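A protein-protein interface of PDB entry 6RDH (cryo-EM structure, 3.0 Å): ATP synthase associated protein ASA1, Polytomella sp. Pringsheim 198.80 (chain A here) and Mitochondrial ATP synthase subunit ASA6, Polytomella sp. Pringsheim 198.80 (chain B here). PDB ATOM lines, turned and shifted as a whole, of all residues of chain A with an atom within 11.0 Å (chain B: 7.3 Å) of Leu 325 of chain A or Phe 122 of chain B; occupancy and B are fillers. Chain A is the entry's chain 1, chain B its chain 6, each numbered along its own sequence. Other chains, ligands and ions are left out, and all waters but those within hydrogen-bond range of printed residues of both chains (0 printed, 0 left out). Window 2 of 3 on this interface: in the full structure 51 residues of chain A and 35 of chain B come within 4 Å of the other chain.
The side-chain hydroxyl (OG) of Ser 323 of chain A lies within hydrogen-bond range of the backbone carbonyl oxygen (O) of Ala 320 of chain A, at 2.9 Å.
Printed residues of chain B within 4 Å of Leu 315 of chain A: Phe 127 (3.6 Å).
Of the printed residues of chain B, Ala 320 of chain A touches Tyr 126.
Of chain B, only Phe 122 comes within 4 Å of Leu 325 of chain A.
Of the printed residues of chain B, Leu 326 of chain A touches Phe 122, Arg 123 and Tyr 126.
Lys 327 of chain A touches none of the printed residues of chain B.
Of the printed residues of chain B, Glu 329 of chain A touches Arg 123.
Phe 116 of chain B touches none of the printed residues of chain A.
No residue of chain A comes within 4 Å of Ser 117 of chain B.
No residue of chain A comes within 4 Å of Ile 120 of chain B.
Of the printed residues of chain A, Phe 122 of chain B touches Leu 325 and Leu 326.
No residue of chain A comes within 4 Å of Val 125 of chain B.
Of the printed residues of chain A, Tyr 126 of chain B touches Ala 320 (3.3 Å), Phe 321 (3.7 Å) and Leu 326 (3.8 Å).
The nearest residue of chain B that does not touch Leu 325 of chain A is Arg 123 of chain B (5.5 Å).
The nearest residue of chain A that does not touch Phe 122 of chain B is Glu 329 of chain A (5.7 Å).
The nearest printed residue of chain B that does not touch Lys 330 of chain A is Phe 127 of chain B (5.3 Å).
OE1 of Glu 334 of chain A lies within salt-bridge range of NE of Arg 123 of chain B.
The side-chain carboxylate (OE2) of Glu 329 of chain A is in salt-bridge range of the guanidinium group (NH1) of Arg 123 of chain B, at 3.0 Å.
CE1 of Phe 127 of chain B touches CD1 of Leu 315 of chain A, 3.6 Å away.
Ala 320 of chain A touches Tyr 126 of chain B (CB to OH, 3.3 Å).
CE2 of Phe 321 of chain A touches CE2 of Tyr 126 of chain B, 3.7 Å away.
CZ of Phe 321 of chain A touches CE2 of Phe 127 of chain B, at 3.8 Å.
Phe 122 of chain B touches Leu 325 of chain A (CE1 to CD1, 3.7 Å).
Leu 326 of chain A touches Phe 122 of chain B.
CA of Arg 123 of chain B touches CD2 of Leu 326 of chain A, 3.7 Å away.
Ala 331 of chain A touches Phe 127 of chain B (CB to CZ, 3.97 Å).
Ser 333 of chain A touches Arg 123 of chain B (CB to NH1, 3.9 Å).
Phe 127 of chain B touches Glu 334 of chain A (CB to OE2, 3.4 Å).
Of the 13 printed residues of chain B, 4 touch a printed residue of chain A.
Of the 16 printed residues of chain A, 10 touch a printed residue of chain B.
Among the printed residues, 14 pairs touch across the chains.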
ATOM      1  N   LEU A 315      27.182  17.778   0.671  1.00  0.00           N
ATOM      2  CA  LEU A 315      25.803  18.227   0.552  1.00  0.00           C
ATOM      3  C   LEU A 315      25.365  18.332  -0.898  1.00  0.00           C
ATOM      4  O   LEU A 315      24.180  18.171  -1.191  1.00  0.00           O
ATOM      5  CB  LEU A 315      25.627  19.581   1.224  1.00  0.00           C
ATOM      6  CG  LEU A 315      25.029  19.632   2.617  1.00  0.00           C
ATOM      7  CD1 LEU A 315      24.797  21.058   2.988  1.00  0.00           C
ATOM      8  CD2 LEU A 315      23.743  18.873   2.654  1.00  0.00           C
ATOM      9  N   PRO A 319      20.620  13.765  -1.650  1.00  0.00           N
ATOM     10  CA  PRO A 319      19.358  13.762  -2.400  1.00  0.00           C
ATOM     11  C   PRO A 319      18.628  15.088  -2.391  1.00  0.00           C
ATOM     12  O   PRO A 319      17.718  15.274  -3.203  1.00  0.00           O
ATOM     13  CB  PRO A 319      18.533  12.692  -1.687  1.00  0.00           C
ATOM     14  CG  PRO A 319      19.510  11.814  -1.082  1.00  0.00           C
ATOM     15  CD  PRO A 319      20.647  12.666  -0.669  1.00  0.00           C
ATOM     16  N   ALA A 320      18.988  16.011  -1.514  1.00  0.00           N
ATOM     17  CA  ALA A 320      18.294  17.281  -1.446  1.00  0.00           C
ATOM     18  C   ALA A 320      18.663  18.206  -2.585  1.00  0.00           C
ATOM     19  O   ALA A 320      17.875  19.083  -2.932  1.00  0.00           O
ATOM     20  CB  ALA A 320      18.601  17.962  -0.124  1.00  0.00           C
ATOM     21  N   PHE A 321      19.846  18.048  -3.162  1.00  0.00           N
ATOM     22  CA  PHE A 321      20.296  18.918  -4.232  1.00  0.00           C
ATOM     23  C   PHE A 321      20.132  18.289  -5.601  1.00  0.00           C
ATOM     24  O   PHE A 321      20.462  18.919  -6.604  1.00  0.00           O
ATOM     25  CB  PHE A 321      21.744  19.332  -4.000  1.00  0.00           C
ATOM     26  CG  PHE A 321      21.877  20.493  -3.079  1.00  0.00           C
ATOM     27  CD1 PHE A 321      22.017  21.765  -3.576  1.00  0.00           C
ATOM     28  CD2 PHE A 321      21.827  20.319  -1.717  1.00  0.00           C
ATOM     29  CE1 PHE A 321      22.120  22.833  -2.735  1.00  0.00           C
ATOM     30  CE2 PHE A 321      21.931  21.391  -0.877  1.00  0.00           C
ATOM     31  CZ  PHE A 321      22.074  22.645  -1.389  1.00  0.00           C
ATOM     32  N   SER A 322      19.638  17.064  -5.665  1.00  0.00           N
ATOM     33  CA  SER A 322      19.132  16.491  -6.898  1.00  0.00           C
ATOM     34  C   SER A 322      17.631  16.668  -7.039  1.00  0.00           C
ATOM     35  O   SER A 322      17.054  16.186  -8.014  1.00  0.00           O
ATOM     36  CB  SER A 322      19.482  15.007  -6.973  1.00  0.00           C
ATOM     37  OG  SER A 322      20.880  14.817  -6.862  1.00  0.00           O
ATOM     38  N   SER A 323      16.985  17.330  -6.085  1.00  0.00           N
ATOM     39  CA  SER A 323      15.580  17.656  -6.222  1.00  0.00           C
ATOM     40  C   SER A 323      15.422  18.839  -7.156  1.00  0.00           C
ATOM     41  O   SER A 323      16.393  19.482  -7.544  1.00  0.00           O
ATOM     42  CB  SER A 323      14.958  17.983  -4.877  1.00  0.00           C
ATOM     43  OG  SER A 323      15.445  19.222  -4.425  1.00  0.00           O
ATOM     44  N   PHE A 324      14.171  19.154  -7.485  1.00  0.00           N
ATOM     45  CA  PHE A 324      13.909  20.069  -8.586  1.00  0.00           C
ATOM     46  C   PHE A 324      14.245  21.507  -8.222  1.00  0.00           C
ATOM     47  O   PHE A 324      14.935  22.198  -8.976  1.00  0.00           O
ATOM     48  CB  PHE A 324      12.456  19.957  -9.020  1.00  0.00           C
ATOM     49  CG  PHE A 324      12.119  20.841 -10.166  1.00  0.00           C
ATOM     50  CD1 PHE A 324      12.549  20.522 -11.436  1.00  0.00           C
ATOM     51  CD2 PHE A 324      11.392  21.999  -9.976  1.00  0.00           C
ATOM     52  CE1 PHE A 324      12.260  21.331 -12.489  1.00  0.00           C
ATOM     53  CE2 PHE A 324      11.102  22.810 -11.028  1.00  0.00           C
ATOM     54  CZ  PHE A 324      11.535  22.476 -12.287  1.00  0.00           C
ATOM     55  N   LEU A 325      13.781  21.976  -7.068  1.00  0.00           N
ATOM     56  CA  LEU A 325      13.956  23.376  -6.707  1.00  0.00           C
ATOM     57  C   LEU A 325      15.376  23.719  -6.289  1.00  0.00           C
ATOM     58  O   LEU A 325      15.685  24.902  -6.144  1.00  0.00           O
ATOM     59  CB  LEU A 325      12.996  23.743  -5.584  1.00  0.00           C
ATOM     60  CG  LEU A 325      11.521  23.488  -5.873  1.00  0.00           C
ATOM     61  CD1 LEU A 325      10.691  23.799  -4.659  1.00  0.00           C
ATOM     62  CD2 LEU A 325      11.074  24.325  -7.042  1.00  0.00           C
ATOM     63  N   LEU A 326      16.240  22.729  -6.105  1.00  0.00           N
ATOM     64  CA  LEU A 326      17.616  22.943  -5.682  1.00  0.00           C
ATOM     65  C   LEU A 326      18.594  22.326  -6.663  1.00  0.00           C
ATOM     66  O   LEU A 326      19.710  21.975  -6.294  1.00  0.00           O
ATOM     67  CB  LEU A 326      17.850  22.365  -4.292  1.00  0.00           C
ATOM     68  CG  LEU A 326      17.226  23.093  -3.123  1.00  0.00           C
ATOM     69  CD1 LEU A 326      17.176  22.163  -1.970  1.00  0.00           C
ATOM     70  CD2 LEU A 326      18.066  24.265  -2.792  1.00  0.00           C
ATOM     71  N   LYS A 327      18.184  22.185  -7.918  1.00  0.00           N
ATOM     72  CA  LYS A 327      18.971  21.428  -8.877  1.00  0.00           C
ATOM     73  C   LYS A 327      20.081  22.267  -9.490  1.00  0.00           C
ATOM     74  O   LYS A 327      21.154  21.738  -9.787  1.00  0.00           O
ATOM     75  CB  LYS A 327      18.044  20.876  -9.951  1.00  0.00           C
ATOM     76  CG  LYS A 327      18.603  19.751 -10.754  1.00  0.00           C
ATOM     77  CD  LYS A 327      17.549  19.239 -11.701  1.00  0.00           C
ATOM     78  CE  LYS A 327      16.481  18.482 -10.957  1.00  0.00           C
ATOM     79  NZ  LYS A 327      15.485  17.884 -11.879  1.00  0.00           N
ATOM     80  N   ARG A 328      19.854  23.561  -9.677  1.00  0.00           N
ATOM     81  CA  ARG A 328      20.870  24.465 -10.199  1.00  0.00           C
ATOM     82  C   ARG A 328      21.741  25.074  -9.115  1.00  0.00           C
ATOM     83  O   ARG A 328      22.765  25.678  -9.437  1.00  0.00           O
ATOM     84  CB  ARG A 328      20.218  25.596 -10.991  1.00  0.00           C
ATOM     85  CG  ARG A 328      19.501  25.155 -12.242  1.00  0.00           C
ATOM     86  CD  ARG A 328      20.437  24.959 -13.402  1.00  0.00           C
ATOM     87  NE  ARG A 328      19.710  24.720 -14.641  1.00  0.00           N
ATOM     88  CZ  ARG A 328      19.313  23.519 -15.042  1.00  0.00           C
ATOM     89  NH1 ARG A 328      19.571  22.454 -14.297  1.00  0.00           N
ATOM     90  NH2 ARG A 328      18.663  23.380 -16.186  1.00  0.00           N
ATOM     91  N   GLU A 329      21.362  24.940  -7.852  1.00  0.00           N
ATOM     92  CA  GLU A 329      22.057  25.601  -6.762  1.00  0.00           C
ATOM     93  C   GLU A 329      23.265  24.786  -6.321  1.00  0.00           C
ATOM     94  O   GLU A 329      23.443  23.627  -6.697  1.00  0.00           O
ATOM     95  CB  GLU A 329      21.117  25.825  -5.583  1.00  0.00           C
ATOM     96  CG  GLU A 329      19.924  26.694  -5.895  1.00  0.00           C
ATOM     97  CD  GLU A 329      20.309  28.003  -6.545  1.00  0.00           C
ATOM     98  OE1 GLU A 329      19.796  28.295  -7.644  1.00  0.00           O
ATOM     99  OE2 GLU A 329      21.128  28.742  -5.963  1.00  0.00           O
ATOM    100  N   LYS A 330      24.114  25.419  -5.521  1.00  0.00           N
ATOM    101  CA  LYS A 330      25.286  24.770  -4.967  1.00  0.00           C
ATOM    102  C   LYS A 330      25.360  25.065  -3.479  1.00  0.00           C
ATOM    103  O   LYS A 330      25.082  26.184  -3.047  1.00  0.00           O
ATOM    104  CB  LYS A 330      26.561  25.239  -5.665  1.00  0.00           C
ATOM    105  CG  LYS A 330      26.718  24.700  -7.071  1.00  0.00           C
ATOM    106  CD  LYS A 330      26.712  23.189  -7.067  1.00  0.00           C
ATOM    107  CE  LYS A 330      26.628  22.625  -8.467  1.00  0.00           C
ATOM    108  NZ  LYS A 330      26.535  21.141  -8.441  1.00  0.00           N
ATOM    109  N   ALA A 331      25.736  24.053  -2.701  1.00  0.00           N
ATOM    110  CA  ALA A 331      25.851  24.201  -1.260  1.00  0.00           C
ATOM    111  C   ALA A 331      27.068  25.008  -0.857  1.00  0.00           C
ATOM    112  O   ALA A 331      27.148  25.452   0.292  1.00  0.00           O
ATOM    113  CB  ALA A 331      25.905  22.831  -0.597  1.00  0.00           C
ATOM    114  N   SER A 333      27.551  27.856  -2.143  1.00  0.00           N
ATOM    115  CA  SER A 333      27.080  29.228  -2.235  1.00  0.00           C
ATOM    116  C   SER A 333      26.548  29.750  -0.914  1.00  0.00           C
ATOM    117  O   SER A 333      26.547  30.966  -0.705  1.00  0.00           O
ATOM    118  CB  SER A 333      25.988  29.342  -3.294  1.00  0.00           C
ATOM    119  OG  SER A 333      26.487  29.009  -4.571  1.00  0.00           O
ATOM    120  N   GLU A 334      26.085  28.876  -0.024  1.00  0.00           N
ATOM    121  CA  GLU A 334      25.511  29.365   1.222  1.00  0.00           C
ATOM    122  C   GLU A 334      26.598  29.697   2.234  1.00  0.00           C
ATOM    123  O   GLU A 334      26.743  30.854   2.641  1.00  0.00           O
ATOM    124  CB  GLU A 334      24.526  28.347   1.787  1.00  0.00           C
ATOM    125  CG  GLU A 334      23.908  28.764   3.117  1.00  0.00           C
ATOM    126  CD  GLU A 334      22.721  29.713   2.983  1.00  0.00           C
ATOM    127  OE1 GLU A 334      22.384  30.125   1.854  1.00  0.00           O
ATOM    128  OE2 GLU A 334      22.115  30.044   4.022  1.00  0.00           O
ATOM    129  N   PHE B 116       5.214  32.508  -6.208  1.00  0.00           N
ATOM    130  CA  PHE B 116       6.025  31.915  -5.156  1.00  0.00           C
ATOM    131  C   PHE B 116       7.090  30.998  -5.713  1.00  0.00           C
ATOM    132  O   PHE B 116       8.178  30.914  -5.147  1.00  0.00           O
ATOM    133  CB  PHE B 116       5.148  31.157  -4.172  1.00  0.00           C
ATOM    134  CG  PHE B 116       4.518  32.023  -3.143  1.00  0.00           C
ATOM    135  CD1 PHE B 116       5.056  33.260  -2.852  1.00  0.00           C
ATOM    136  CD2 PHE B 116       3.398  31.613  -2.472  1.00  0.00           C
ATOM    137  CE1 PHE B 116       4.489  34.066  -1.906  1.00  0.00           C
ATOM    138  CE2 PHE B 116       2.830  32.420  -1.536  1.00  0.00           C
ATOM    139  CZ  PHE B 116       3.376  33.647  -1.250  1.00  0.00           C
ATOM    140  N   SER B 117       6.835  30.340  -6.835  1.00  0.00           N
ATOM    141  CA  SER B 117       7.897  29.532  -7.418  1.00  0.00           C
ATOM    142  C   SER B 117       8.921  30.348  -8.196  1.00  0.00           C
ATOM    143  O   SER B 117       9.704  29.761  -8.941  1.00  0.00           O
ATOM    144  CB  SER B 117       7.315  28.460  -8.332  1.00  0.00           C
ATOM    145  OG  SER B 117       6.728  29.049  -9.470  1.00  0.00           O
ATOM    146  N   SER B 118       8.931  31.672  -8.060  1.00  0.00           N
ATOM    147  CA  SER B 118       9.808  32.525  -8.834  1.00  0.00           C
ATOM    148  C   SER B 118      10.578  33.543  -8.012  1.00  0.00           C
ATOM    149  O   SER B 118      11.609  34.027  -8.481  1.00  0.00           O
ATOM    150  CB  SER B 118       8.998  33.277  -9.897  1.00  0.00           C
ATOM    151  OG  SER B 118       9.811  34.202 -10.583  1.00  0.00           O
ATOM    152  N   LEU B 119      10.126  33.879  -6.807  1.00  0.00           N
ATOM    153  CA  LEU B 119      10.847  34.835  -5.983  1.00  0.00           C
ATOM    154  C   LEU B 119      11.271  34.293  -4.627  1.00  0.00           C
ATOM    155  O   LEU B 119      12.040  34.962  -3.932  1.00  0.00           O
ATOM    156  CB  LEU B 119      10.020  36.116  -5.803  1.00  0.00           C
ATOM    157  CG  LEU B 119       8.614  36.119  -5.206  1.00  0.00           C
ATOM    158  CD1 LEU B 119       8.570  36.306  -3.690  1.00  0.00           C
ATOM    159  CD2 LEU B 119       7.803  37.190  -5.904  1.00  0.00           C
ATOM    160  N   ILE B 120      10.787  33.123  -4.231  1.00  0.00           N
ATOM    161  CA  ILE B 120      11.275  32.479  -3.007  1.00  0.00           C
ATOM    162  C   ILE B 120      12.701  31.993  -3.237  1.00  0.00           C
ATOM    163  O   ILE B 120      12.957  31.297  -4.231  1.00  0.00           O
ATOM    164  CB  ILE B 120      10.361  31.318  -2.613  1.00  0.00           C
ATOM    165  CG1 ILE B 120       9.018  31.835  -2.118  1.00  0.00           C
ATOM    166  CG2 ILE B 120      10.987  30.479  -1.536  1.00  0.00           C
ATOM    167  CD1 ILE B 120       8.055  30.736  -1.738  1.00  0.00           C
ATOM    168  N   PRO B 121      13.660  32.347  -2.380  1.00  0.00           N
ATOM    169  CA  PRO B 121      15.000  31.753  -2.462  1.00  0.00           C
ATOM    170  C   PRO B 121      14.992  30.355  -1.870  1.00  0.00           C
ATOM    171  O   PRO B 121      14.809  30.177  -0.664  1.00  0.00           O
ATOM    172  CB  PRO B 121      15.857  32.721  -1.638  1.00  0.00           C
ATOM    173  CG  PRO B 121      14.919  33.387  -0.721  1.00  0.00           C
ATOM    174  CD  PRO B 121      13.590  33.428  -1.384  1.00  0.00           C
ATOM    175  N   PHE B 122      15.177  29.351  -2.718  1.00  0.00           N
ATOM    176  CA  PHE B 122      15.002  27.990  -2.234  1.00  0.00           C
ATOM    177  C   PHE B 122      16.249  27.442  -1.566  1.00  0.00           C
ATOM    178  O   PHE B 122      16.141  26.567  -0.705  1.00  0.00           O
ATOM    179  CB  PHE B 122      14.557  27.090  -3.371  1.00  0.00           C
ATOM    180  CG  PHE B 122      13.151  27.327  -3.781  1.00  0.00           C
ATOM    181  CD1 PHE B 122      12.116  27.001  -2.933  1.00  0.00           C
ATOM    182  CD2 PHE B 122      12.860  27.903  -5.000  1.00  0.00           C
ATOM    183  CE1 PHE B 122      10.817  27.232  -3.295  1.00  0.00           C
ATOM    184  CE2 PHE B 122      11.560  28.134  -5.369  1.00  0.00           C
ATOM    185  CZ  PHE B 122      10.538  27.796  -4.514  1.00  0.00           C
ATOM    186  N   ARG B 123      17.429  27.942  -1.917  1.00  0.00           N
ATOM    187  CA  ARG B 123      18.617  27.539  -1.181  1.00  0.00           C
ATOM    188  C   ARG B 123      18.649  28.185   0.194  1.00  0.00           C
ATOM    189  O   ARG B 123      19.065  27.556   1.170  1.00  0.00           O
ATOM    190  CB  ARG B 123      19.871  27.888  -1.971  1.00  0.00           C
ATOM    191  CG  ARG B 123      21.131  27.272  -1.429  1.00  0.00           C
ATOM    192  CD  ARG B 123      22.346  28.006  -1.925  1.00  0.00           C
ATOM    193  NE  ARG B 123      22.367  29.383  -1.453  1.00  0.00           N
ATOM    194  CZ  ARG B 123      22.281  30.442  -2.246  1.00  0.00           C
ATOM    195  NH1 ARG B 123      22.180  30.284  -3.555  1.00  0.00           N
ATOM    196  NH2 ARG B 123      22.300  31.659  -1.731  1.00  0.00           N
ATOM    197  N   ALA B 124      18.193  29.431   0.292  1.00  0.00           N
ATOM    198  CA  ALA B 124      18.129  30.082   1.590  1.00  0.00           C
ATOM    199  C   ALA B 124      17.066  29.446   2.466  1.00  0.00           C
ATOM    200  O   ALA B 124      17.264  29.295   3.672  1.00  0.00           O
ATOM    201  CB  ALA B 124      17.856  31.568   1.418  1.00  0.00           C
ATOM    202  N   VAL B 125      15.949  29.032   1.871  1.00  0.00           N
ATOM    203  CA  VAL B 125      14.905  28.344   2.621  1.00  0.00           C
ATOM    204  C   VAL B 125      15.375  26.962   3.052  1.00  0.00           C
ATOM    205  O   VAL B 125      15.091  26.527   4.173  1.00  0.00           O
ATOM    206  CB  VAL B 125      13.617  28.305   1.782  1.00  0.00           C
ATOM    207  CG1 VAL B 125      12.697  27.178   2.179  1.00  0.00           C
ATOM    208  CG2 VAL B 125      12.890  29.605   1.942  1.00  0.00           C
ATOM    209  N   TYR B 126      16.158  26.282   2.209  1.00  0.00           N
ATOM    210  CA  TYR B 126      16.717  24.986   2.581  1.00  0.00           C
ATOM    211  C   TYR B 126      17.683  25.110   3.749  1.00  0.00           C
ATOM    212  O   TYR B 126      17.560  24.397   4.748  1.00  0.00           O
ATOM    213  CB  TYR B 126      17.424  24.355   1.390  1.00  0.00           C
ATOM    214  CG  TYR B 126      18.027  23.019   1.713  1.00  0.00           C
ATOM    215  CD1 TYR B 126      17.230  21.905   1.850  1.00  0.00           C
ATOM    216  CD2 TYR B 126      19.387  22.873   1.891  1.00  0.00           C
ATOM    217  CE1 TYR B 126      17.764  20.687   2.157  1.00  0.00           C
ATOM    218  CE2 TYR B 126      19.928  21.657   2.204  1.00  0.00           C
ATOM    219  CZ  TYR B 126      19.111  20.571   2.330  1.00  0.00           C
ATOM    220  OH  TYR B 126      19.649  19.353   2.641  1.00  0.00           O
ATOM    221  N   PHE B 127      18.631  26.031   3.660  1.00  0.00           N
ATOM    222  CA  PHE B 127      19.584  26.187   4.747  1.00  0.00           C
ATOM    223  C   PHE B 127      19.016  26.933   5.939  1.00  0.00           C
ATOM    224  O   PHE B 127      19.688  27.013   6.968  1.00  0.00           O
ATOM    225  CB  PHE B 127      20.834  26.891   4.248  1.00  0.00           C
ATOM    226  CG  PHE B 127      21.750  26.001   3.496  1.00  0.00           C
ATOM    227  CD1 PHE B 127      22.649  25.205   4.159  1.00  0.00           C
ATOM    228  CD2 PHE B 127      21.696  25.942   2.124  1.00  0.00           C
ATOM    229  CE1 PHE B 127      23.480  24.383   3.465  1.00  0.00           C
ATOM    230  CE2 PHE B 127      22.526  25.116   1.429  1.00  0.00           C
ATOM    231  CZ  PHE B 127      23.417  24.339   2.099  1.00  0.00           C
ATOM    232  N   ALA B 128      17.815  27.490   5.834  1.00  0.00           N
ATOM    233  CA  ALA B 128      17.170  28.088   6.988  1.00  0.00           C
ATOM    234  C   ALA B 128      16.285  27.100   7.717  1.00  0.00           C
ATOM    235  O   ALA B 128      16.143  27.193   8.935  1.00  0.00           O
ATOM    236  CB  ALA B 128      16.345  29.301   6.565  1.00  0.00           C
